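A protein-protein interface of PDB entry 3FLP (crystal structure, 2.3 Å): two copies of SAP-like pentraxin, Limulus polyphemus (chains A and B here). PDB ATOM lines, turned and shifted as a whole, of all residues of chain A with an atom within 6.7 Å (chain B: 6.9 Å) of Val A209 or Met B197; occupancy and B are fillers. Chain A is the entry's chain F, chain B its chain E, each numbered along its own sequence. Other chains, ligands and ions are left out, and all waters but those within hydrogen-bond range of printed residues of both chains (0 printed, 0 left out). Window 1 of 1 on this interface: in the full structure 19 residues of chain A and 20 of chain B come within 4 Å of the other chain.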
ATOM      1  N   VAL A   2     -17.936  -4.598  18.197  1.00  0.00           N
ATOM      2  CA  VAL A   2     -18.625  -4.951  19.432  1.00  0.00           C
ATOM      3  C   VAL A   2     -19.891  -4.125  19.617  1.00  0.00           C
ATOM      4  O   VAL A   2     -19.853  -2.893  19.582  1.00  0.00           O
ATOM      5  CB  VAL A   2     -17.716  -4.741  20.644  1.00  0.00           C
ATOM      6  CG1 VAL A   2     -18.427  -5.190  21.904  1.00  0.00           C
ATOM      7  CG2 VAL A   2     -16.426  -5.507  20.450  1.00  0.00           C
ATOM      8  N   ILE A   4     -23.082  -2.535  21.640  1.00  0.00           N
ATOM      9  CA  ILE A   4     -23.310  -1.986  22.962  1.00  0.00           C
ATOM     10  C   ILE A   4     -24.171  -2.890  23.858  1.00  0.00           C
ATOM     11  O   ILE A   4     -24.098  -2.814  25.086  1.00  0.00           O
ATOM     12  CB  ILE A   4     -23.944  -0.595  22.838  1.00  0.00           C
ATOM     13  CG1 ILE A   4     -23.732   0.180  24.129  1.00  0.00           C
ATOM     14  CG2 ILE A   4     -25.417  -0.712  22.506  1.00  0.00           C
ATOM     15  CD1 ILE A   4     -24.086   1.644  23.996  1.00  0.00           C
ATOM     16  N   VAL A   7     -22.129  -5.137  26.325  1.00  0.00           N
ATOM     17  CA  VAL A   7     -21.327  -4.564  27.398  1.00  0.00           C
ATOM     18  C   VAL A   7     -21.826  -5.252  28.666  1.00  0.00           C
ATOM     19  O   VAL A   7     -23.018  -5.519  28.802  1.00  0.00           O
ATOM     20  CB  VAL A   7     -21.547  -3.030  27.529  1.00  0.00           C
ATOM     21  CG1 VAL A   7     -20.967  -2.520  28.851  1.00  0.00           C
ATOM     22  CG2 VAL A   7     -20.884  -2.311  26.366  1.00  0.00           C
ATOM     23  N   LYS A   8     -20.926  -5.556  29.587  1.00  0.00           N
ATOM     24  CA  LYS A   8     -21.344  -6.215  30.817  1.00  0.00           C
ATOM     25  C   LYS A   8     -20.807  -5.497  32.041  1.00  0.00           C
ATOM     26  O   LYS A   8     -19.836  -4.741  31.961  1.00  0.00           O
ATOM     27  CB  LYS A   8     -20.858  -7.667  30.845  1.00  0.00           C
ATOM     28  CG  LYS A   8     -19.379  -7.819  31.173  1.00  0.00           C
ATOM     29  CD  LYS A   8     -18.981  -9.284  31.199  1.00  0.00           C
ATOM     30  CE  LYS A   8     -17.509  -9.459  31.552  1.00  0.00           C
ATOM     31  NZ  LYS A   8     -17.092 -10.877  31.408  1.00  0.00           N
ATOM     32  N   ILE A   9     -21.460  -5.733  33.171  1.00  0.00           N
ATOM     33  CA  ILE A   9     -21.044  -5.153  34.434  1.00  0.00           C
ATOM     34  C   ILE A   9     -20.814  -6.307  35.401  1.00  0.00           C
ATOM     35  O   ILE A   9     -21.658  -7.203  35.529  1.00  0.00           O
ATOM     36  CB  ILE A   9     -22.122  -4.239  35.042  1.00  0.00           C
ATOM     37  CG1 ILE A   9     -22.413  -3.053  34.111  1.00  0.00           C
ATOM     38  CG2 ILE A   9     -21.652  -3.748  36.410  1.00  0.00           C
ATOM     39  CD1 ILE A   9     -21.211  -2.177  33.820  1.00  0.00           C
ATOM     40  N   SER A  10     -19.666  -6.295  36.066  1.00  0.00           N
ATOM     41  CA  SER A  10     -19.353  -7.320  37.038  1.00  0.00           C
ATOM     42  C   SER A  10     -19.559  -6.759  38.445  1.00  0.00           C
ATOM     43  O   SER A  10     -19.053  -5.680  38.772  1.00  0.00           O
ATOM     44  CB  SER A  10     -17.897  -7.774  36.889  1.00  0.00           C
ATOM     45  OG  SER A  10     -17.710  -8.532  35.707  1.00  0.00           O
ATOM     46  N   MET A 197     -27.474   0.356  28.290  1.00  0.00           N
ATOM     47  CA  MET A 197     -26.487   1.329  27.826  1.00  0.00           C
ATOM     48  C   MET A 197     -27.076   2.522  27.063  1.00  0.00           C
ATOM     49  O   MET A 197     -26.332   3.311  26.475  1.00  0.00           O
ATOM     50  CB  MET A 197     -25.429   0.645  26.953  1.00  0.00           C
ATOM     51  CG  MET A 197     -24.685  -0.502  27.635  1.00  0.00           C
ATOM     52  SD  MET A 197     -23.915  -0.024  29.206  1.00  0.00           S
ATOM     53  CE  MET A 197     -22.641   1.100  28.649  1.00  0.00           C
ATOM     54  N   PHE A 201     -26.857   5.466  34.043  1.00  0.00           N
ATOM     55  CA  PHE A 201     -26.863   4.923  35.387  1.00  0.00           C
ATOM     56  C   PHE A 201     -25.551   5.229  36.085  1.00  0.00           C
ATOM     57  O   PHE A 201     -24.504   5.355  35.444  1.00  0.00           O
ATOM     58  CB  PHE A 201     -27.130   3.409  35.366  1.00  0.00           C
ATOM     59  CG  PHE A 201     -26.123   2.606  34.573  1.00  0.00           C
ATOM     60  CD1 PHE A 201     -24.885   2.276  35.116  1.00  0.00           C
ATOM     61  CD2 PHE A 201     -26.426   2.166  33.288  1.00  0.00           C
ATOM     62  CE1 PHE A 201     -23.967   1.515  34.391  1.00  0.00           C
ATOM     63  CE2 PHE A 201     -25.514   1.405  32.554  1.00  0.00           C
ATOM     64  CZ  PHE A 201     -24.285   1.078  33.101  1.00  0.00           C
ATOM     65  N   ALA A 203     -22.490   4.213  38.432  1.00  0.00           N
ATOM     66  CA  ALA A 203     -21.744   2.990  38.746  1.00  0.00           C
ATOM     67  C   ALA A 203     -20.998   3.304  40.031  1.00  0.00           C
ATOM     68  O   ALA A 203     -20.342   4.344  40.128  1.00  0.00           O
ATOM     69  CB  ALA A 203     -20.757   2.675  37.631  1.00  0.00           C
ATOM     70  N   VAL A 207     -17.727  -1.634  40.593  1.00  0.00           N
ATOM     71  CA  VAL A 207     -18.271  -2.544  39.591  1.00  0.00           C
ATOM     72  C   VAL A 207     -17.274  -2.507  38.439  1.00  0.00           C
ATOM     73  O   VAL A 207     -16.562  -1.511  38.257  1.00  0.00           O
ATOM     74  CB  VAL A 207     -19.677  -2.119  39.100  1.00  0.00           C
ATOM     75  CG1 VAL A 207     -20.698  -2.343  40.219  1.00  0.00           C
ATOM     76  CG2 VAL A 207     -19.671  -0.656  38.658  1.00  0.00           C
ATOM     77  N   ILE A 208     -17.203  -3.594  37.678  1.00  0.00           N
ATOM     78  CA  ILE A 208     -16.262  -3.671  36.575  1.00  0.00           C
ATOM     79  C   ILE A 208     -16.978  -3.642  35.235  1.00  0.00           C
ATOM     80  O   ILE A 208     -17.891  -4.430  34.996  1.00  0.00           O
ATOM     81  CB  ILE A 208     -15.421  -4.952  36.672  1.00  0.00           C
ATOM     82  CG1 ILE A 208     -14.759  -5.025  38.046  1.00  0.00           C
ATOM     83  CG2 ILE A 208     -14.366  -4.973  35.583  1.00  0.00           C
ATOM     84  CD1 ILE A 208     -13.982  -6.294  38.276  1.00  0.00           C
ATOM     85  N   VAL A 209     -16.565  -2.717  34.372  1.00  0.00           N
ATOM     86  CA  VAL A 209     -17.148  -2.584  33.040  1.00  0.00           C
ATOM     87  C   VAL A 209     -16.317  -3.418  32.064  1.00  0.00           C
ATOM     88  O   VAL A 209     -15.102  -3.241  31.966  1.00  0.00           O
ATOM     89  CB  VAL A 209     -17.130  -1.112  32.528  1.00  0.00           C
ATOM     90  CG1 VAL A 209     -17.845  -1.026  31.163  1.00  0.00           C
ATOM     91  CG2 VAL A 209     -17.788  -0.177  33.543  1.00  0.00           C
ATOM     92  N   GLY A 210     -16.980  -4.319  31.344  1.00  0.00           N
ATOM     93  CA  GLY A 210     -16.290  -5.162  30.385  1.00  0.00           C
ATOM     94  C   GLY A 210     -17.213  -5.611  29.267  1.00  0.00           C
ATOM     95  O   GLY A 210     -18.229  -4.968  28.990  1.00  0.00           O
ATOM     96  N   ILE A 211     -16.865  -6.721  28.624  1.00  0.00           N
ATOM     97  CA  ILE A 211     -17.669  -7.258  27.533  1.00  0.00           C
ATOM     98  C   ILE A 211     -18.159  -8.672  27.829  1.00  0.00           C
ATOM     99  O   ILE A 211     -17.423  -9.508  28.349  1.00  0.00           O
ATOM    100  CB  ILE A 211     -16.876  -7.312  26.207  1.00  0.00           C
ATOM    101  CG1 ILE A 211     -16.504  -5.896  25.744  1.00  0.00           C
ATOM    102  CG2 ILE A 211     -17.705  -8.027  25.143  1.00  0.00           C
ATOM    103  CD1 ILE A 211     -17.700  -5.000  25.407  1.00  0.00           C
ATOM    104  N   ILE B   4     -20.575   1.163  20.513  1.00  0.00           N
ATOM    105  CA  ILE B   4     -19.886   1.111  21.787  1.00  0.00           C
ATOM    106  C   ILE B   4     -18.840   2.221  21.955  1.00  0.00           C
ATOM    107  O   ILE B   4     -18.502   2.602  23.076  1.00  0.00           O
ATOM    108  CB  ILE B   4     -19.242  -0.284  21.977  1.00  0.00           C
ATOM    109  CG1 ILE B   4     -19.138  -0.602  23.462  1.00  0.00           C
ATOM    110  CG2 ILE B   4     -17.869  -0.344  21.316  1.00  0.00           C
ATOM    111  CD1 ILE B   4     -18.697  -2.013  23.733  1.00  0.00           C
ATOM    112  N   ARG B   5     -18.349   2.753  20.840  1.00  0.00           N
ATOM    113  CA  ARG B   5     -17.357   3.820  20.882  1.00  0.00           C
ATOM    114  C   ARG B   5     -17.957   5.137  21.349  1.00  0.00           C
ATOM    115  O   ARG B   5     -17.224   6.044  21.723  1.00  0.00           O
ATOM    116  CB  ARG B   5     -16.691   3.990  19.510  1.00  0.00           C
ATOM    117  CG  ARG B   5     -15.580   2.962  19.246  1.00  0.00           C
ATOM    118  CD  ARG B   5     -15.190   2.850  17.763  1.00  0.00           C
ATOM    119  NE  ARG B   5     -16.303   2.364  16.953  1.00  0.00           N
ATOM    120  CZ  ARG B   5     -16.190   1.890  15.715  1.00  0.00           C
ATOM    121  NH1 ARG B   5     -15.003   1.830  15.119  1.00  0.00           N
ATOM    122  NH2 ARG B   5     -17.271   1.465  15.074  1.00  0.00           N
ATOM    123  N   ASP B   6     -19.284   5.232  21.350  1.00  0.00           N
ATOM    124  CA  ASP B   6     -19.957   6.449  21.780  1.00  0.00           C
ATOM    125  C   ASP B   6     -20.427   6.414  23.235  1.00  0.00           C
ATOM    126  O   ASP B   6     -21.090   7.350  23.696  1.00  0.00           O
ATOM    127  CB  ASP B   6     -21.136   6.775  20.848  1.00  0.00           C
ATOM    128  CG  ASP B   6     -20.678   7.236  19.461  1.00  0.00           C
ATOM    129  OD1 ASP B   6     -19.841   8.162  19.388  1.00  0.00           O
ATOM    130  OD2 ASP B   6     -21.159   6.679  18.446  1.00  0.00           O
ATOM    131  N   VAL B   7     -20.100   5.342  23.954  1.00  0.00           N
ATOM    132  CA  VAL B   7     -20.459   5.250  25.369  1.00  0.00           C
ATOM    133  C   VAL B   7     -19.617   6.318  26.064  1.00  0.00           C
ATOM    134  O   VAL B   7     -18.459   6.530  25.702  1.00  0.00           O
ATOM    135  CB  VAL B   7     -20.104   3.852  25.970  1.00  0.00           C
ATOM    136  CG1 VAL B   7     -20.176   3.890  27.508  1.00  0.00           C
ATOM    137  CG2 VAL B   7     -21.068   2.800  25.440  1.00  0.00           C
ATOM    138  N   LYS B   8     -20.187   7.007  27.045  1.00  0.00           N
ATOM    139  CA  LYS B   8     -19.424   8.030  27.744  1.00  0.00           C
ATOM    140  C   LYS B   8     -19.492   7.835  29.248  1.00  0.00           C
ATOM    141  O   LYS B   8     -20.391   7.165  29.762  1.00  0.00           O
ATOM    142  CB  LYS B   8     -19.948   9.423  27.403  1.00  0.00           C
ATOM    143  CG  LYS B   8     -21.262   9.770  28.091  1.00  0.00           C
ATOM    144  CD  LYS B   8     -21.727  11.163  27.724  1.00  0.00           C
ATOM    145  CE  LYS B   8     -22.987  11.538  28.491  1.00  0.00           C
ATOM    146  NZ  LYS B   8     -23.478  12.856  28.053  1.00  0.00           N
ATOM    147  N   ILE B   9     -18.519   8.411  29.942  1.00  0.00           N
ATOM    148  CA  ILE B   9     -18.468   8.350  31.394  1.00  0.00           C
ATOM    149  C   ILE B   9     -18.435   9.795  31.887  1.00  0.00           C
ATOM    150  O   ILE B   9     -17.658  10.614  31.387  1.00  0.00           O
ATOM    151  CB  ILE B   9     -17.185   7.640  31.922  1.00  0.00           C
ATOM    152  CG1 ILE B   9     -17.107   6.192  31.413  1.00  0.00           C
ATOM    153  CG2 ILE B   9     -17.163   7.690  33.451  1.00  0.00           C
ATOM    154  CD1 ILE B   9     -18.233   5.279  31.852  1.00  0.00           C
ATOM    155  N   LEU B  22     -11.908   5.888  37.037  1.00  0.00           N
ATOM    156  CA  LEU B  22     -11.898   4.594  36.380  1.00  0.00           C
ATOM    157  C   LEU B  22     -10.490   4.057  36.592  1.00  0.00           C
ATOM    158  O   LEU B  22      -9.541   4.829  36.656  1.00  0.00           O
ATOM    159  CB  LEU B  22     -12.117   4.734  34.879  1.00  0.00           C
ATOM    160  CG  LEU B  22     -13.357   5.429  34.338  1.00  0.00           C
ATOM    161  CD1 LEU B  22     -13.345   5.290  32.817  1.00  0.00           C
ATOM    162  CD2 LEU B  22     -14.612   4.815  34.926  1.00  0.00           C
ATOM    163  N   PHE B  24      -8.188   0.850  34.976  1.00  0.00           N
ATOM    164  CA  PHE B  24      -8.149  -0.301  34.095  1.00  0.00           C
ATOM    165  C   PHE B  24      -7.625  -1.539  34.810  1.00  0.00           C
ATOM    166  O   PHE B  24      -6.637  -1.477  35.542  1.00  0.00           O
ATOM    167  CB  PHE B  24      -7.331   0.034  32.850  1.00  0.00           C
ATOM    168  CG  PHE B  24      -8.086   0.875  31.868  1.00  0.00           C
ATOM    169  CD1 PHE B  24      -8.220   2.246  32.062  1.00  0.00           C
ATOM    170  CD2 PHE B  24      -8.741   0.281  30.790  1.00  0.00           C
ATOM    171  CE1 PHE B  24      -9.003   3.020  31.198  1.00  0.00           C
ATOM    172  CE2 PHE B  24      -9.529   1.046  29.917  1.00  0.00           C
ATOM    173  CZ  PHE B  24      -9.659   2.417  30.126  1.00  0.00           C
ATOM    174  N   MET B  25      -8.321  -2.654  34.607  1.00  0.00           N
ATOM    175  CA  MET B  25      -7.989  -3.934  35.226  1.00  0.00           C
ATOM    176  C   MET B  25      -6.633  -4.503  34.835  1.00  0.00           C
ATOM    177  O   MET B  25      -5.955  -5.119  35.654  1.00  0.00           O
ATOM    178  CB  MET B  25      -9.071  -4.963  34.880  1.00  0.00           C
ATOM    179  CG  MET B  25     -10.445  -4.649  35.452  1.00  0.00           C
ATOM    180  SD  MET B  25     -10.421  -4.608  37.258  1.00  0.00           S
ATOM    181  CE  MET B  25     -10.398  -6.378  37.620  1.00  0.00           C
ATOM    182  N   ASP B 165     -14.767   7.501  23.921  1.00  0.00           N
ATOM    183  CA  ASP B 165     -13.877   7.093  22.835  1.00  0.00           C
ATOM    184  C   ASP B 165     -12.380   7.164  23.171  1.00  0.00           C
ATOM    185  O   ASP B 165     -11.595   7.707  22.388  1.00  0.00           O
ATOM    186  CB  ASP B 165     -14.162   7.977  21.620  1.00  0.00           C
ATOM    187  CG  ASP B 165     -14.096   7.221  20.304  1.00  0.00           C
ATOM    188  OD1 ASP B 165     -13.491   6.129  20.260  1.00  0.00           O
ATOM    189  OD2 ASP B 165     -14.643   7.740  19.305  1.00  0.00           O
ATOM    190  N   LEU B 166     -11.990   6.629  24.326  1.00  0.00           N
ATOM    191  CA  LEU B 166     -10.580   6.628  24.722  1.00  0.00           C
ATOM    192  C   LEU B 166      -9.845   5.545  23.943  1.00  0.00           C
ATOM    193  O   LEU B 166     -10.186   4.361  24.035  1.00  0.00           O
ATOM    194  CB  LEU B 166     -10.433   6.350  26.222  1.00  0.00           C
ATOM    195  CG  LEU B 166      -9.010   6.174  26.764  1.00  0.00           C
ATOM    196  CD1 LEU B 166      -8.234   7.480  26.614  1.00  0.00           C
ATOM    197  CD2 LEU B 166      -9.069   5.766  28.235  1.00  0.00           C
ATOM    198  N   GLN B 167      -8.843   5.953  23.173  1.00  0.00           N
ATOM    199  CA  GLN B 167      -8.057   5.019  22.376  1.00  0.00           C
ATOM    200  C   GLN B 167      -6.566   5.278  22.632  1.00  0.00           C
ATOM    201  O   GLN B 167      -6.099   6.411  22.510  1.00  0.00           O
ATOM    202  CB  GLN B 167      -8.366   5.212  20.891  1.00  0.00           C
ATOM    203  CG  GLN B 167      -9.847   5.159  20.513  1.00  0.00           C
ATOM    204  CD  GLN B 167     -10.517   3.836  20.862  1.00  0.00           C
ATOM    205  OE1 GLN B 167      -9.853   2.812  21.042  1.00  0.00           O
ATOM    206  NE2 GLN B 167     -11.844   3.850  20.939  1.00  0.00           N
ATOM    207  N   ILE B 194      -5.184   0.268  24.590  1.00  0.00           N
ATOM    208  CA  ILE B 194      -6.492   0.404  25.220  1.00  0.00           C
ATOM    209  C   ILE B 194      -7.500   0.784  24.144  1.00  0.00           C
ATOM    210  O   ILE B 194      -7.303   1.750  23.405  1.00  0.00           O
ATOM    211  CB  ILE B 194      -6.517   1.494  26.328  1.00  0.00           C
ATOM    212  CG1 ILE B 194      -5.860   0.966  27.604  1.00  0.00           C
ATOM    213  CG2 ILE B 194      -7.973   1.918  26.634  1.00  0.00           C
ATOM    214  CD1 ILE B 194      -5.782   2.000  28.696  1.00  0.00           C
ATOM    215  N   SER B 195      -8.564  -0.006  24.045  1.00  0.00           N
ATOM    216  CA  SER B 195      -9.637   0.248  23.097  1.00  0.00           C
ATOM    217  C   SER B 195     -10.875   0.501  23.957  1.00  0.00           C
ATOM    218  O   SER B 195     -11.277  -0.370  24.728  1.00  0.00           O
ATOM    219  CB  SER B 195      -9.855  -0.972  22.200  1.00  0.00           C
ATOM    220  OG  SER B 195     -10.952  -0.760  21.325  1.00  0.00           O
ATOM    221  N   TRP B 196     -11.465   1.687  23.828  1.00  0.00           N
ATOM    222  CA  TRP B 196     -12.639   2.061  24.618  1.00  0.00           C
ATOM    223  C   TRP B 196     -13.718   0.978  24.687  1.00  0.00           C
ATOM    224  O   TRP B 196     -14.197   0.491  23.661  1.00  0.00           O
ATOM    225  CB  TRP B 196     -13.248   3.354  24.070  1.00  0.00           C
ATOM    226  CG  TRP B 196     -14.288   3.985  24.965  1.00  0.00           C
ATOM    227  CD1 TRP B 196     -15.542   4.384  24.602  1.00  0.00           C
ATOM    228  CD2 TRP B 196     -14.139   4.346  26.348  1.00  0.00           C
ATOM    229  NE1 TRP B 196     -16.186   4.974  25.670  1.00  0.00           N
ATOM    230  CE2 TRP B 196     -15.348   4.965  26.753  1.00  0.00           C
ATOM    231  CE3 TRP B 196     -13.107   4.210  27.283  1.00  0.00           C
ATOM    232  CZ2 TRP B 196     -15.549   5.448  28.053  1.00  0.00           C
ATOM    233  CZ3 TRP B 196     -13.305   4.687  28.576  1.00  0.00           C
ATOM    234  CH2 TRP B 196     -14.520   5.301  28.949  1.00  0.00           C
ATOM    235  N   MET B 197     -14.078   0.607  25.914  1.00  0.00           N
ATOM    236  CA  MET B 197     -15.100  -0.399  26.182  1.00  0.00           C
ATOM    237  C   MET B 197     -14.730  -1.822  25.761  1.00  0.00           C
ATOM    238  O   MET B 197     -15.575  -2.712  25.783  1.00  0.00           O
ATOM    239  CB  MET B 197     -16.420   0.006  25.524  1.00  0.00           C
ATOM    240  CG  MET B 197     -16.953   1.354  25.992  1.00  0.00           C
ATOM    241  SD  MET B 197     -17.203   1.417  27.774  1.00  0.00           S
ATOM    242  CE  MET B 197     -18.626   0.322  27.949  1.00  0.00           C
ATOM    243  N   GLU B 198     -13.480  -2.037  25.366  1.00  0.00           N
ATOM    244  CA  GLU B 198     -13.024  -3.376  24.992  1.00  0.00           C
ATOM    245  C   GLU B 198     -11.976  -3.847  26.000  1.00  0.00           C
ATOM    246  O   GLU B 198     -11.558  -5.000  25.985  1.00  0.00           O
ATOM    247  CB  GLU B 198     -12.439  -3.384  23.577  1.00  0.00           C
ATOM    248  CG  GLU B 198     -13.474  -3.636  22.488  1.00  0.00           C
ATOM    249  CD  GLU B 198     -12.882  -3.608  21.084  1.00  0.00           C
ATOM    250  OE1 GLU B 198     -11.717  -4.033  20.918  1.00  0.00           O
ATOM    251  OE2 GLU B 198     -13.588  -3.178  20.145  1.00  0.00           O
ATOM    252  N   ASP B 199     -11.552  -2.934  26.867  1.00  0.00           N
ATOM    253  CA  ASP B 199     -10.585  -3.228  27.912  1.00  0.00           C
ATOM    254  C   ASP B 199     -11.256  -2.863  29.230  1.00  0.00           C
ATOM    255  O   ASP B 199     -11.588  -1.705  29.477  1.00  0.00           O
ATOM    256  CB  ASP B 199      -9.298  -2.427  27.692  1.00  0.00           C
ATOM    257  CG  ASP B 199      -8.429  -3.032  26.599  1.00  0.00           C
ATOM    258  OD1 ASP B 199      -8.021  -4.206  26.756  1.00  0.00           O
ATOM    259  OD2 ASP B 199      -8.164  -2.352  25.582  1.00  0.00           O
ATOM    260  N   SER B 200     -11.475  -3.878  30.056  1.00  0.00           N
ATOM    261  CA  SER B 200     -12.145  -3.734  31.343  1.00  0.00           C
ATOM    262  C   SER B 200     -11.563  -2.701  32.285  1.00  0.00           C
ATOM    263  O   SER B 200     -10.348  -2.536  32.379  1.00  0.00           O
ATOM    264  CB  SER B 200     -12.160  -5.079  32.070  1.00  0.00           C
ATOM    265  OG  SER B 200     -12.769  -6.067  31.264  1.00  0.00           O
ATOM    266  N   PHE B 201     -12.448  -2.016  32.996  1.00  0.00           N
ATOM    267  CA  PHE B 201     -12.024  -1.025  33.969  1.00  0.00           C
ATOM    268  C   PHE B 201     -13.020  -0.955  35.116  1.00  0.00           C
ATOM    269  O   PHE B 201     -14.214  -1.222  34.943  1.00  0.00           O
ATOM    270  CB  PHE B 201     -11.845   0.352  33.305  1.00  0.00           C
ATOM    271  CG  PHE B 201     -13.092   0.892  32.642  1.00  0.00           C
ATOM    272  CD1 PHE B 201     -14.096   1.504  33.390  1.00  0.00           C
ATOM    273  CD2 PHE B 201     -13.251   0.804  31.264  1.00  0.00           C
ATOM    274  CE1 PHE B 201     -15.235   2.020  32.772  1.00  0.00           C
ATOM    275  CE2 PHE B 201     -14.384   1.314  30.640  1.00  0.00           C
ATOM    276  CZ  PHE B 201     -15.378   1.923  31.390  1.00  0.00           C
ATOM    277  N   VAL B 202     -12.513  -0.626  36.297  1.00  0.00           N
ATOM    278  CA  VAL B 202     -13.352  -0.495  37.474  1.00  0.00           C
ATOM    279  C   VAL B 202     -13.916   0.920  37.478  1.00  0.00           C
ATOM    280  O   VAL B 202     -13.208   1.878  37.169  1.00  0.00           O
ATOM    281  CB  VAL B 202     -12.545  -0.715  38.779  1.00  0.00           C
ATOM    282  CG1 VAL B 202     -13.470  -0.645  39.982  1.00  0.00           C
ATOM    283  CG2 VAL B 202     -11.845  -2.053  38.737  1.00  0.00           C
ATOM    284  N   ALA B 203     -15.198   1.042  37.794  1.00  0.00           N
ATOM    285  CA  ALA B 203     -15.866   2.340  37.864  1.00  0.00           C
ATOM    286  C   ALA B 203     -16.136   2.561  39.350  1.00  0.00           C
ATOM    287  O   ALA B 203     -16.654   1.673  40.027  1.00  0.00           O
ATOM    288  CB  ALA B 203     -17.168   2.308  37.089  1.00  0.00           C
ATOM    289  N   VAL B 209     -22.551   6.383  33.688  1.00  0.00           N
ATOM    290  CA  VAL B 209     -22.427   5.750  32.381  1.00  0.00           C
ATOM    291  C   VAL B 209     -23.592   6.206  31.500  1.00  0.00           C
ATOM    292  O   VAL B 209     -24.767   6.083  31.878  1.00  0.00           O
ATOM    293  CB  VAL B 209     -22.453   4.196  32.485  1.00  0.00           C
ATOM    294  CG1 VAL B 209     -22.236   3.586  31.105  1.00  0.00           C
ATOM    295  CG2 VAL B 209     -21.378   3.708  33.451  1.00  0.00           C
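The backbone carbonyl oxygen (O) of Phe B201 sits at hydrogen-bond distance from the backbone NH (N) of Val A209.
The backbone carbonyl oxygen (O) of Val A207 lies within hydrogen-bond range of the backbone NH (N) of Ala B203, at 2.9 Å.
The backbone carbonyl oxygen (O) of Phe A201 is in hydrogen-bond range of the backbone NH (N) of Val B209 (2.8 Å).
Val A7 touches Met B197, and with the chains exchanged Met A197 touches Val B7.
Met A197 touches Val B209, and with the chains exchanged Val A209 touches Met B197.
Phe A201 touches Val B209, and with the chains exchanged Val A209 touches Phe B201.
Ala B203 touches its own counterpart, Ala A203.
Positions printed for both chains: 4, 7, 8, 9, 197, 201, 203 and 209.
Of the printed residues of chain B, Val A209 touches Met B197, Ser B200 and Phe B201.
Met B197 touches just these residues of chain A: Val A7 (3.8 Å), Val A209 (3.6 Å) and Ile A211 (3.1 Å).
Of the printed residues of chain B, Val A207 touches Val B202 and Ala B203.
Of the printed residues of chain B, Ala A203 touches Ala B203.
Of the printed residues of chain B, Gly A210 touches Ser B200.
Printed residues of chain B within 4 Å of Ile A211: Ile B4 (3.6 Å) and Met B197 (3.1 Å).
Of the printed residues of chain A, Val B202 touches Val A207.
Phe B24 touches none of the printed residues of chain A.
Lys B8 touches none of the printed residues of chain A.
The nearest residue of chain A that does not touch Met B197 is Met A197 (4.1 Å).
The nearest printed residue of chain B that does not touch Ala A203 is Val B209 (4.4 Å).
Of the 14 printed residues of chain A, 11 touch a printed residue of chain B.
Hydrophobic or aromatic side chains of chain A that line the printed part of chain B: Val A2, Ile A4, Val A7, Met A197, Phe A201, Ala A203, Ile A208, Val A209 and Ile A211.
Along chain A the printed residues that touch a printed residue of chain B span positions 2 to 211.
Of the 23 printed residues of chain B, 10 touch a printed residue of chain A.
Hydrophobic or aromatic side chains of chain B within 4 Å of the printed part of chain A: Ile B4, Val B7, Met B25, Met B197, Phe B201, Val B202, Ala B203 and Val B209.
Among the printed residues, no Asp or Glu carboxylate lies within 4 Å of a Lys or Arg side-chain nitrogen of the other chain.
Val A2 touches Glu B198.
Val B7 touches Ile A4.
Val A7 touches Ile B4.
CG1 of Val B7 touches CE of Met A197, 3.9 Å away.
Ala A203 touches Ala B203 (CB to CB, 3.6 Å).
CA of Val B202 touches O of Val A207, at 3.5 Å.
Met B25 touches Ile A208 (CE to CD1, 3.6 Å).
Val A209 touches Met B197 (CG1 to CE, 3.6 Å).
Gly A210 touches Ser B200 (CA to OG, 3.7 Å).
Met B197 touches Ile A211.
The side-chain hydroxyl (OG) of Ser B195 lies within hydrogen-bond range of the side-chain carboxylate (OE1) of Glu B198.
O of Val B7 is in hydrogen-bond range of NE1 of Trp B196 (2.8 Å).
N of Ser A10 is in hydrogen-bond range of O of Ile A208 (2.8 Å).
O of Gly A210 lies within hydrogen-bond range of N of Lys A8 (2.8 Å).
The backbone NH (N) of Met B25 is in hydrogen-bond range of the backbone carbonyl oxygen (O) of Ser B200, 3.0 Å away.
NZ of Lys A8 sits close to O of Ile A211 (3.4 Å).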
